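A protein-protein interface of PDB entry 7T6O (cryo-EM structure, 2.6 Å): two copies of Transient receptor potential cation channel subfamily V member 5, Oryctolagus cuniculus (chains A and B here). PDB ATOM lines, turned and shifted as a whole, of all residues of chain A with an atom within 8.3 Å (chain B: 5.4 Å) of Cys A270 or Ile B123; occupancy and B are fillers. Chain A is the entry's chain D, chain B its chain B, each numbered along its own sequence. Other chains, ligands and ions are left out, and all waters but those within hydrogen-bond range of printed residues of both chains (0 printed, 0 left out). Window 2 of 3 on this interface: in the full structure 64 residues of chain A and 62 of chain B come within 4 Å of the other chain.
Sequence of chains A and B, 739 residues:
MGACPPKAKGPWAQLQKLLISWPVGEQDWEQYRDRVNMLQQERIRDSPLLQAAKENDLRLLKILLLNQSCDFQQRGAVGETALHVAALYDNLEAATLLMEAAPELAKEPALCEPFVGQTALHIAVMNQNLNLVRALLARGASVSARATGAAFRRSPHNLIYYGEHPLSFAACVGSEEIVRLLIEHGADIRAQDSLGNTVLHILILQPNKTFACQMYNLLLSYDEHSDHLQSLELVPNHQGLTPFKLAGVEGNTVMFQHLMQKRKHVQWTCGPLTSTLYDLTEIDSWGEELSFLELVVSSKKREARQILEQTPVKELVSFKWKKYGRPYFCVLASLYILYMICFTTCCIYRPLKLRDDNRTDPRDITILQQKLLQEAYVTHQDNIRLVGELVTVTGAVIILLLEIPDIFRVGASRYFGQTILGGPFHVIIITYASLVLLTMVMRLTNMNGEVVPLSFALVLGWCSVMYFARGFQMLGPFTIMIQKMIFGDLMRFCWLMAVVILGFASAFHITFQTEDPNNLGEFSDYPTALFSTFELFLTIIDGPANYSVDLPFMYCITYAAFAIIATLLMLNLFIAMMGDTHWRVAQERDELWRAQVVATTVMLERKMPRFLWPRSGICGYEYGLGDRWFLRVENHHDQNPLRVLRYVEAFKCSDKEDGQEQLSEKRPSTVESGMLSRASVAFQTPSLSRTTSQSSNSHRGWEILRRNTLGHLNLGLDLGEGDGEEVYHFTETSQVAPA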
ATOM      1  N   VAL A 266     -25.308  29.677  -9.746  1.00  0.00           N
ATOM      2  CA  VAL A 266     -24.608  29.209 -10.936  1.00  0.00           C
ATOM      3  C   VAL A 266     -25.637  28.797 -11.978  1.00  0.00           C
ATOM      4  O   VAL A 266     -26.465  27.910 -11.738  1.00  0.00           O
ATOM      5  CB  VAL A 266     -23.661  28.051 -10.596  1.00  0.00           C
ATOM      6  CG1 VAL A 266     -23.059  27.471 -11.864  1.00  0.00           C
ATOM      7  CG2 VAL A 266     -22.567  28.524  -9.655  1.00  0.00           C
ATOM      8  N   GLN A 267     -25.596  29.449 -13.139  1.00  0.00           N
ATOM      9  CA  GLN A 267     -26.561  29.169 -14.195  1.00  0.00           C
ATOM     10  C   GLN A 267     -26.233  27.866 -14.909  1.00  0.00           C
ATOM     11  O   GLN A 267     -27.028  26.920 -14.899  1.00  0.00           O
ATOM     12  CB  GLN A 267     -26.597  30.327 -15.191  1.00  0.00           C
ATOM     13  CG  GLN A 267     -27.285  31.566 -14.673  1.00  0.00           C
ATOM     14  CD  GLN A 267     -27.417  32.626 -15.737  1.00  0.00           C
ATOM     15  OE1 GLN A 267     -26.466  33.345 -16.038  1.00  0.00           O
ATOM     16  NE2 GLN A 267     -28.597  32.721 -16.326  1.00  0.00           N
ATOM     17  N   TRP A 268     -25.061  27.801 -15.534  1.00  0.00           N
ATOM     18  CA  TRP A 268     -24.634  26.593 -16.222  1.00  0.00           C
ATOM     19  C   TRP A 268     -23.117  26.543 -16.237  1.00  0.00           C
ATOM     20  O   TRP A 268     -22.434  27.551 -16.027  1.00  0.00           O
ATOM     21  CB  TRP A 268     -25.190  26.520 -17.650  1.00  0.00           C
ATOM     22  CG  TRP A 268     -25.113  27.809 -18.419  1.00  0.00           C
ATOM     23  CD1 TRP A 268     -26.119  28.710 -18.603  1.00  0.00           C
ATOM     24  CD2 TRP A 268     -23.977  28.328 -19.125  1.00  0.00           C
ATOM     25  NE1 TRP A 268     -25.681  29.762 -19.366  1.00  0.00           N
ATOM     26  CE2 TRP A 268     -24.370  29.551 -19.703  1.00  0.00           C
ATOM     27  CE3 TRP A 268     -22.667  27.878 -19.324  1.00  0.00           C
ATOM     28  CZ2 TRP A 268     -23.499  30.332 -20.461  1.00  0.00           C
ATOM     29  CZ3 TRP A 268     -21.805  28.655 -20.075  1.00  0.00           C
ATOM     30  CH2 TRP A 268     -22.224  29.868 -20.634  1.00  0.00           C
ATOM     31  N   THR A 269     -22.603  25.341 -16.486  1.00  0.00           N
ATOM     32  CA  THR A 269     -21.179  25.104 -16.689  1.00  0.00           C
ATOM     33  C   THR A 269     -21.028  24.320 -17.983  1.00  0.00           C
ATOM     34  O   THR A 269     -21.250  23.105 -18.008  1.00  0.00           O
ATOM     35  CB  THR A 269     -20.565  24.345 -15.514  1.00  0.00           C
ATOM     36  OG1 THR A 269     -20.887  25.014 -14.289  1.00  0.00           O
ATOM     37  CG2 THR A 269     -19.054  24.270 -15.662  1.00  0.00           C
ATOM     38  N   CYS A 270     -20.662  25.014 -19.054  1.00  0.00           N
ATOM     39  CA  CYS A 270     -20.434  24.404 -20.358  1.00  0.00           C
ATOM     40  C   CYS A 270     -18.931  24.391 -20.601  1.00  0.00           C
ATOM     41  O   CYS A 270     -18.333  25.438 -20.881  1.00  0.00           O
ATOM     42  CB  CYS A 270     -21.169  25.165 -21.457  1.00  0.00           C
ATOM     43  SG  CYS A 270     -21.483  24.196 -22.948  1.00  0.00           S
ATOM     44  N   GLY A 271     -18.330  23.206 -20.487  1.00  0.00           N
ATOM     45  CA  GLY A 271     -16.906  23.038 -20.643  1.00  0.00           C
ATOM     46  C   GLY A 271     -16.119  23.793 -19.594  1.00  0.00           C
ATOM     47  O   GLY A 271     -16.309  23.613 -18.387  1.00  0.00           O
ATOM     48  N   PRO A 272     -15.211  24.665 -20.041  1.00  0.00           N
ATOM     49  CA  PRO A 272     -14.505  25.543 -19.101  1.00  0.00           C
ATOM     50  C   PRO A 272     -15.297  26.776 -18.701  1.00  0.00           C
ATOM     51  O   PRO A 272     -14.900  27.460 -17.748  1.00  0.00           O
ATOM     52  CB  PRO A 272     -13.248  25.932 -19.881  1.00  0.00           C
ATOM     53  CG  PRO A 272     -13.707  25.949 -21.298  1.00  0.00           C
ATOM     54  CD  PRO A 272     -14.728  24.842 -21.423  1.00  0.00           C
ATOM     55  N   LEU A 273     -16.396  27.081 -19.388  1.00  0.00           N
ATOM     56  CA  LEU A 273     -17.139  28.308 -19.140  1.00  0.00           C
ATOM     57  C   LEU A 273     -18.205  28.084 -18.076  1.00  0.00           C
ATOM     58  O   LEU A 273     -18.907  27.072 -18.087  1.00  0.00           O
ATOM     59  CB  LEU A 273     -17.783  28.815 -20.429  1.00  0.00           C
ATOM     60  CG  LEU A 273     -16.884  28.806 -21.667  1.00  0.00           C
ATOM     61  CD1 LEU A 273     -17.702  29.017 -22.930  1.00  0.00           C
ATOM     62  CD2 LEU A 273     -15.791  29.856 -21.544  1.00  0.00           C
ATOM     63  N   THR A 274     -18.309  29.029 -17.149  1.00  0.00           N
ATOM     64  CA  THR A 274     -19.308  28.988 -16.093  1.00  0.00           C
ATOM     65  C   THR A 274     -20.026  30.328 -16.035  1.00  0.00           C
ATOM     66  O   THR A 274     -19.383  31.379 -15.962  1.00  0.00           O
ATOM     67  CB  THR A 274     -18.666  28.674 -14.734  1.00  0.00           C
ATOM     68  OG1 THR A 274     -18.045  27.384 -14.786  1.00  0.00           O
ATOM     69  CG2 THR A 274     -19.708  28.672 -13.625  1.00  0.00           C
ATOM     70  N   SER A 275     -21.356  30.293 -16.073  1.00  0.00           N
ATOM     71  CA  SER A 275     -22.175  31.493 -15.945  1.00  0.00           C
ATOM     72  C   SER A 275     -22.789  31.515 -14.552  1.00  0.00           C
ATOM     73  O   SER A 275     -23.416  30.536 -14.133  1.00  0.00           O
ATOM     74  CB  SER A 275     -23.262  31.533 -17.016  1.00  0.00           C
ATOM     75  OG  SER A 275     -24.078  32.680 -16.875  1.00  0.00           O
ATOM     76  N   GLU A 634     -19.573  35.548 -16.427  1.00  0.00           N
ATOM     77  CA  GLU A 634     -19.149  34.343 -17.123  1.00  0.00           C
ATOM     78  C   GLU A 634     -17.633  34.251 -17.025  1.00  0.00           C
ATOM     79  O   GLU A 634     -16.922  35.144 -17.496  1.00  0.00           O
ATOM     80  CB  GLU A 634     -19.606  34.353 -18.581  1.00  0.00           C
ATOM     81  CG  GLU A 634     -19.347  33.046 -19.311  1.00  0.00           C
ATOM     82  CD  GLU A 634     -20.151  32.920 -20.590  1.00  0.00           C
ATOM     83  OE1 GLU A 634     -21.152  33.650 -20.740  1.00  0.00           O
ATOM     84  OE2 GLU A 634     -19.780  32.090 -21.446  1.00  0.00           O
ATOM     85  N   ASN A 635     -17.146  33.179 -16.412  1.00  0.00           N
ATOM     86  CA  ASN A 635     -15.725  33.010 -16.163  1.00  0.00           C
ATOM     87  C   ASN A 635     -15.225  31.708 -16.777  1.00  0.00           C
ATOM     88  O   ASN A 635     -15.994  30.782 -17.049  1.00  0.00           O
ATOM     89  CB  ASN A 635     -15.410  33.040 -14.660  1.00  0.00           C
ATOM     90  CG  ASN A 635     -16.248  32.060 -13.865  1.00  0.00           C
ATOM     91  OD1 ASN A 635     -17.476  32.134 -13.862  1.00  0.00           O
ATOM     92  ND2 ASN A 635     -15.584  31.136 -13.181  1.00  0.00           N
ATOM     93  N   HIS A 636     -13.917  31.662 -17.005  1.00  0.00           N
ATOM     94  CA  HIS A 636     -13.244  30.507 -17.578  1.00  0.00           C
ATOM     95  C   HIS A 636     -12.304  29.913 -16.541  1.00  0.00           C
ATOM     96  O   HIS A 636     -11.467  30.625 -15.977  1.00  0.00           O
ATOM     97  CB  HIS A 636     -12.470  30.901 -18.841  1.00  0.00           C
ATOM     98  CG  HIS A 636     -11.299  30.017 -19.140  1.00  0.00           C
ATOM     99  ND1 HIS A 636     -11.430  28.792 -19.757  1.00  0.00           N
ATOM    100  CD2 HIS A 636      -9.974  30.187 -18.920  1.00  0.00           C
ATOM    101  CE1 HIS A 636     -10.238  28.240 -19.896  1.00  0.00           C
ATOM    102  NE2 HIS A 636      -9.337  29.066 -19.396  1.00  0.00           N
ATOM    103  N   HIS A 637     -12.445  28.609 -16.287  1.00  0.00           N
ATOM    104  CA  HIS A 637     -11.602  27.889 -15.332  1.00  0.00           C
ATOM    105  C   HIS A 637     -11.083  26.632 -16.029  1.00  0.00           C
ATOM    106  O   HIS A 637     -11.686  25.561 -15.903  1.00  0.00           O
ATOM    107  CB  HIS A 637     -12.378  27.562 -14.053  1.00  0.00           C
ATOM    108  CG  HIS A 637     -11.507  27.223 -12.883  1.00  0.00           C
ATOM    109  ND1 HIS A 637     -11.637  27.841 -11.658  1.00  0.00           N
ATOM    110  CD2 HIS A 637     -10.499  26.329 -12.748  1.00  0.00           C
ATOM    111  CE1 HIS A 637     -10.745  27.345 -10.820  1.00  0.00           C
ATOM    112  NE2 HIS A 637     -10.041  26.426 -11.456  1.00  0.00           N
ATOM    113  N   HIS B  84     -30.339  20.128 -26.790  1.00  0.00           N
ATOM    114  CA  HIS B  84     -29.285  21.073 -26.432  1.00  0.00           C
ATOM    115  C   HIS B  84     -29.332  21.421 -24.949  1.00  0.00           C
ATOM    116  O   HIS B  84     -28.289  21.537 -24.297  1.00  0.00           O
ATOM    117  CB  HIS B  84     -29.414  22.351 -27.259  1.00  0.00           C
ATOM    118  CG  HIS B  84     -29.195  22.162 -28.727  1.00  0.00           C
ATOM    119  ND1 HIS B  84     -30.062  21.447 -29.524  1.00  0.00           N
ATOM    120  CD2 HIS B  84     -28.223  22.623 -29.548  1.00  0.00           C
ATOM    121  CE1 HIS B  84     -29.627  21.463 -30.771  1.00  0.00           C
ATOM    122  NE2 HIS B  84     -28.513  22.171 -30.812  1.00  0.00           N
ATOM    123  N   ALA B  87     -28.112  18.434 -23.007  1.00  0.00           N
ATOM    124  CA  ALA B  87     -26.661  18.298 -23.100  1.00  0.00           C
ATOM    125  C   ALA B  87     -25.945  19.398 -22.323  1.00  0.00           C
ATOM    126  O   ALA B  87     -24.808  19.207 -21.878  1.00  0.00           O
ATOM    127  CB  ALA B  87     -26.228  18.310 -24.565  1.00  0.00           C
ATOM    128  N   LEU B  88     -26.590  20.558 -22.164  1.00  0.00           N
ATOM    129  CA  LEU B  88     -25.958  21.676 -21.471  1.00  0.00           C
ATOM    130  C   LEU B  88     -25.845  21.416 -19.973  1.00  0.00           C
ATOM    131  O   LEU B  88     -24.813  21.714 -19.360  1.00  0.00           O
ATOM    132  CB  LEU B  88     -26.744  22.961 -21.736  1.00  0.00           C
ATOM    133  CG  LEU B  88     -26.318  24.243 -21.014  1.00  0.00           C
ATOM    134  CD1 LEU B  88     -24.857  24.565 -21.274  1.00  0.00           C
ATOM    135  CD2 LEU B  88     -27.202  25.407 -21.425  1.00  0.00           C
ATOM    136  N   GLN B 118     -24.471  25.796 -33.623  1.00  0.00           N
ATOM    137  CA  GLN B 118     -24.226  24.900 -32.501  1.00  0.00           C
ATOM    138  C   GLN B 118     -25.229  23.755 -32.489  1.00  0.00           C
ATOM    139  O   GLN B 118     -26.442  23.967 -32.544  1.00  0.00           O
ATOM    140  CB  GLN B 118     -24.305  25.655 -31.175  1.00  0.00           C
ATOM    141  CG  GLN B 118     -23.868  24.817 -29.984  1.00  0.00           C
ATOM    142  CD  GLN B 118     -24.146  25.489 -28.657  1.00  0.00           C
ATOM    143  OE1 GLN B 118     -25.189  26.113 -28.473  1.00  0.00           O
ATOM    144  NE2 GLN B 118     -23.211  25.366 -27.724  1.00  0.00           N
ATOM    145  N   THR B 119     -24.713  22.534 -32.406  1.00  0.00           N
ATOM    146  CA  THR B 119     -25.529  21.342 -32.247  1.00  0.00           C
ATOM    147  C   THR B 119     -25.337  20.785 -30.843  1.00  0.00           C
ATOM    148  O   THR B 119     -24.517  21.274 -30.061  1.00  0.00           O
ATOM    149  CB  THR B 119     -25.181  20.278 -33.297  1.00  0.00           C
ATOM    150  OG1 THR B 119     -23.897  19.714 -33.006  1.00  0.00           O
ATOM    151  CG2 THR B 119     -25.162  20.886 -34.688  1.00  0.00           C
ATOM    152  N   ALA B 120     -26.115  19.748 -30.525  1.00  0.00           N
ATOM    153  CA  ALA B 120     -25.973  19.090 -29.230  1.00  0.00           C
ATOM    154  C   ALA B 120     -24.685  18.281 -29.156  1.00  0.00           C
ATOM    155  O   ALA B 120     -24.179  18.020 -28.056  1.00  0.00           O
ATOM    156  CB  ALA B 120     -27.180  18.195 -28.959  1.00  0.00           C
ATOM    157  N   LEU B 121     -24.150  17.876 -30.312  1.00  0.00           N
ATOM    158  CA  LEU B 121     -22.862  17.192 -30.349  1.00  0.00           C
ATOM    159  C   LEU B 121     -21.736  18.111 -29.894  1.00  0.00           C
ATOM    160  O   LEU B 121     -20.810  17.663 -29.212  1.00  0.00           O
ATOM    161  CB  LEU B 121     -22.591  16.655 -31.755  1.00  0.00           C
ATOM    162  CG  LEU B 121     -21.306  15.846 -31.953  1.00  0.00           C
ATOM    163  CD1 LEU B 121     -21.255  14.663 -30.999  1.00  0.00           C
ATOM    164  CD2 LEU B 121     -21.176  15.383 -33.394  1.00  0.00           C
ATOM    165  N   HIS B 122     -21.813  19.399 -30.249  1.00  0.00           N
ATOM    166  CA  HIS B 122     -20.828  20.381 -29.795  1.00  0.00           C
ATOM    167  C   HIS B 122     -20.831  20.511 -28.276  1.00  0.00           C
ATOM    168  O   HIS B 122     -19.770  20.533 -27.639  1.00  0.00           O
ATOM    169  CB  HIS B 122     -21.114  21.741 -30.432  1.00  0.00           C
ATOM    170  CG  HIS B 122     -20.695  21.847 -31.865  1.00  0.00           C
ATOM    171  ND1 HIS B 122     -21.600  21.853 -32.904  1.00  0.00           N
ATOM    172  CD2 HIS B 122     -19.472  21.971 -32.430  1.00  0.00           C
ATOM    173  CE1 HIS B 122     -20.951  21.968 -34.048  1.00  0.00           C
ATOM    174  NE2 HIS B 122     -19.659  22.042 -33.789  1.00  0.00           N
ATOM    175  N   ILE B 123     -22.024  20.576 -27.678  1.00  0.00           N
ATOM    176  CA  ILE B 123     -22.144  20.718 -26.230  1.00  0.00           C
ATOM    177  C   ILE B 123     -21.696  19.444 -25.523  1.00  0.00           C
ATOM    178  O   ILE B 123     -21.049  19.501 -24.469  1.00  0.00           O
ATOM    179  CB  ILE B 123     -23.589  21.093 -25.854  1.00  0.00           C
ATOM    180  CG1 ILE B 123     -24.115  22.187 -26.781  1.00  0.00           C
ATOM    181  CG2 ILE B 123     -23.659  21.553 -24.417  1.00  0.00           C
ATOM    182  CD1 ILE B 123     -25.584  22.482 -26.599  1.00  0.00           C
ATOM    183  N   ALA B 124     -22.028  18.281 -26.091  1.00  0.00           N
ATOM    184  CA  ALA B 124     -21.612  17.011 -25.500  1.00  0.00           C
ATOM    185  C   ALA B 124     -20.102  16.823 -25.587  1.00  0.00           C
ATOM    186  O   ALA B 124     -19.486  16.258 -24.675  1.00  0.00           O
ATOM    187  CB  ALA B 124     -22.336  15.856 -26.189  1.00  0.00           C
ATOM    188  N   VAL B 125     -19.493  17.282 -26.681  1.00  0.00           N
ATOM    189  CA  VAL B 125     -18.046  17.199 -26.839  1.00  0.00           C
ATOM    190  C   VAL B 125     -17.341  18.155 -25.879  1.00  0.00           C
ATOM    191  O   VAL B 125     -16.362  17.782 -25.218  1.00  0.00           O
ATOM    192  CB  VAL B 125     -17.678  17.465 -28.314  1.00  0.00           C
ATOM    193  CG1 VAL B 125     -16.255  17.908 -28.453  1.00  0.00           C
ATOM    194  CG2 VAL B 125     -17.898  16.214 -29.147  1.00  0.00           C
ATOM    195  N   MET B 126     -17.847  19.389 -25.759  1.00  0.00           N
ATOM    196  CA  MET B 126     -17.215  20.377 -24.887  1.00  0.00           C
ATOM    197  C   MET B 126     -17.403  20.022 -23.413  1.00  0.00           C
ATOM    198  O   MET B 126     -16.538  20.321 -22.580  1.00  0.00           O
ATOM    199  CB  MET B 126     -17.769  21.769 -25.207  1.00  0.00           C
ATOM    200  CG  MET B 126     -17.143  22.921 -24.429  1.00  0.00           C
ATOM    201  SD  MET B 126     -17.192  24.488 -25.322  1.00  0.00           S
ATOM    202  CE  MET B 126     -18.951  24.707 -25.559  1.00  0.00           C
ATOM    203  N   ASN B 127     -18.506  19.349 -23.075  1.00  0.00           N
ATOM    204  CA  ASN B 127     -18.719  18.893 -21.706  1.00  0.00           C
ATOM    205  C   ASN B 127     -17.954  17.617 -21.373  1.00  0.00           C
ATOM    206  O   ASN B 127     -17.969  17.209 -20.206  1.00  0.00           O
ATOM    207  CB  ASN B 127     -20.210  18.679 -21.450  1.00  0.00           C
ATOM    208  CG  ASN B 127     -20.901  19.932 -20.951  1.00  0.00           C
ATOM    209  OD1 ASN B 127     -20.303  20.745 -20.247  1.00  0.00           O
ATOM    210  ND2 ASN B 127     -22.167  20.094 -21.313  1.00  0.00           N
ATOM    211  N   GLN B 128     -17.308  16.988 -22.369  1.00  0.00           N
ATOM    212  CA  GLN B 128     -16.463  15.795 -22.210  1.00  0.00           C
ATOM    213  C   GLN B 128     -17.228  14.612 -21.616  1.00  0.00           C
ATOM    214  O   GLN B 128     -16.756  13.946 -20.692  1.00  0.00           O
ATOM    215  CB  GLN B 128     -15.207  16.095 -21.384  1.00  0.00           C
ATOM    216  CG  GLN B 128     -14.263  17.090 -22.023  1.00  0.00           C
ATOM    217  CD  GLN B 128     -13.047  17.368 -21.165  1.00  0.00           C
ATOM    218  OE1 GLN B 128     -12.144  16.539 -21.063  1.00  0.00           O
ATOM    219  NE2 GLN B 128     -13.018  18.538 -20.540  1.00  0.00           N
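OD1 of Asn B127 sits close to O of Thr A269.
The side-chain amide oxygen (OD1) of Asn B127 lies within hydrogen-bond range of the backbone NH (N) of Gly A271, at 3.2 Å.
The backbone carbonyl oxygen (O) of Ala B87 is in hydrogen-bond range of the side-chain amide nitrogen (ND2) of Asn B127, at 2.8 Å.
The side-chain amide nitrogen of Asn B127 sits close to the backbone carbonyl oxygen of Ile B123 (3.4 Å).
Cys A270 touches just these residues of chain B: Leu B88, Ile B123, Met B126 and Asn B127.
Of chain A, only Cys A270 comes within 4 Å of Ile B123.
Of the printed residues of chain A, Asn B127 touches Thr A269 (3.4 Å), Cys A270 (3.7 Å) and Gly A271 (3.2 Å).
Printed residues of chain B within 4 Å of Thr A269: Asn B127 (3.4 Å).
Pro A272 touches none of the printed residues of chain B.
The nearest residue of chain B that does not touch Cys A270 is Gln B118 (5.2 Å).
The nearest residue of chain A that does not touch Ile B123 is Gly A271 (6.1 Å).
CB of Cys A270 touches CD1 of Leu B88, at 3.7 Å.
SG of Cys A270 touches CG2 of Ile B123, at 3.7 Å.
CE of Met B126 touches SG of Cys A270, at 3.7 Å.
OD1 of Asn B127 touches CA of Cys A270, 3.7 Å away.
Gly A271 touches Met B126.
No position is printed for both chains.
Of the 7 pairs that touch across the chains among the printed residues, none has its exchanged pair printed and touching as well.
Of the 14 printed residues of chain B, 4 touch a printed residue of chain A.
Along chain B the printed residues that touch a printed residue of chain A span positions 88 to 127.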
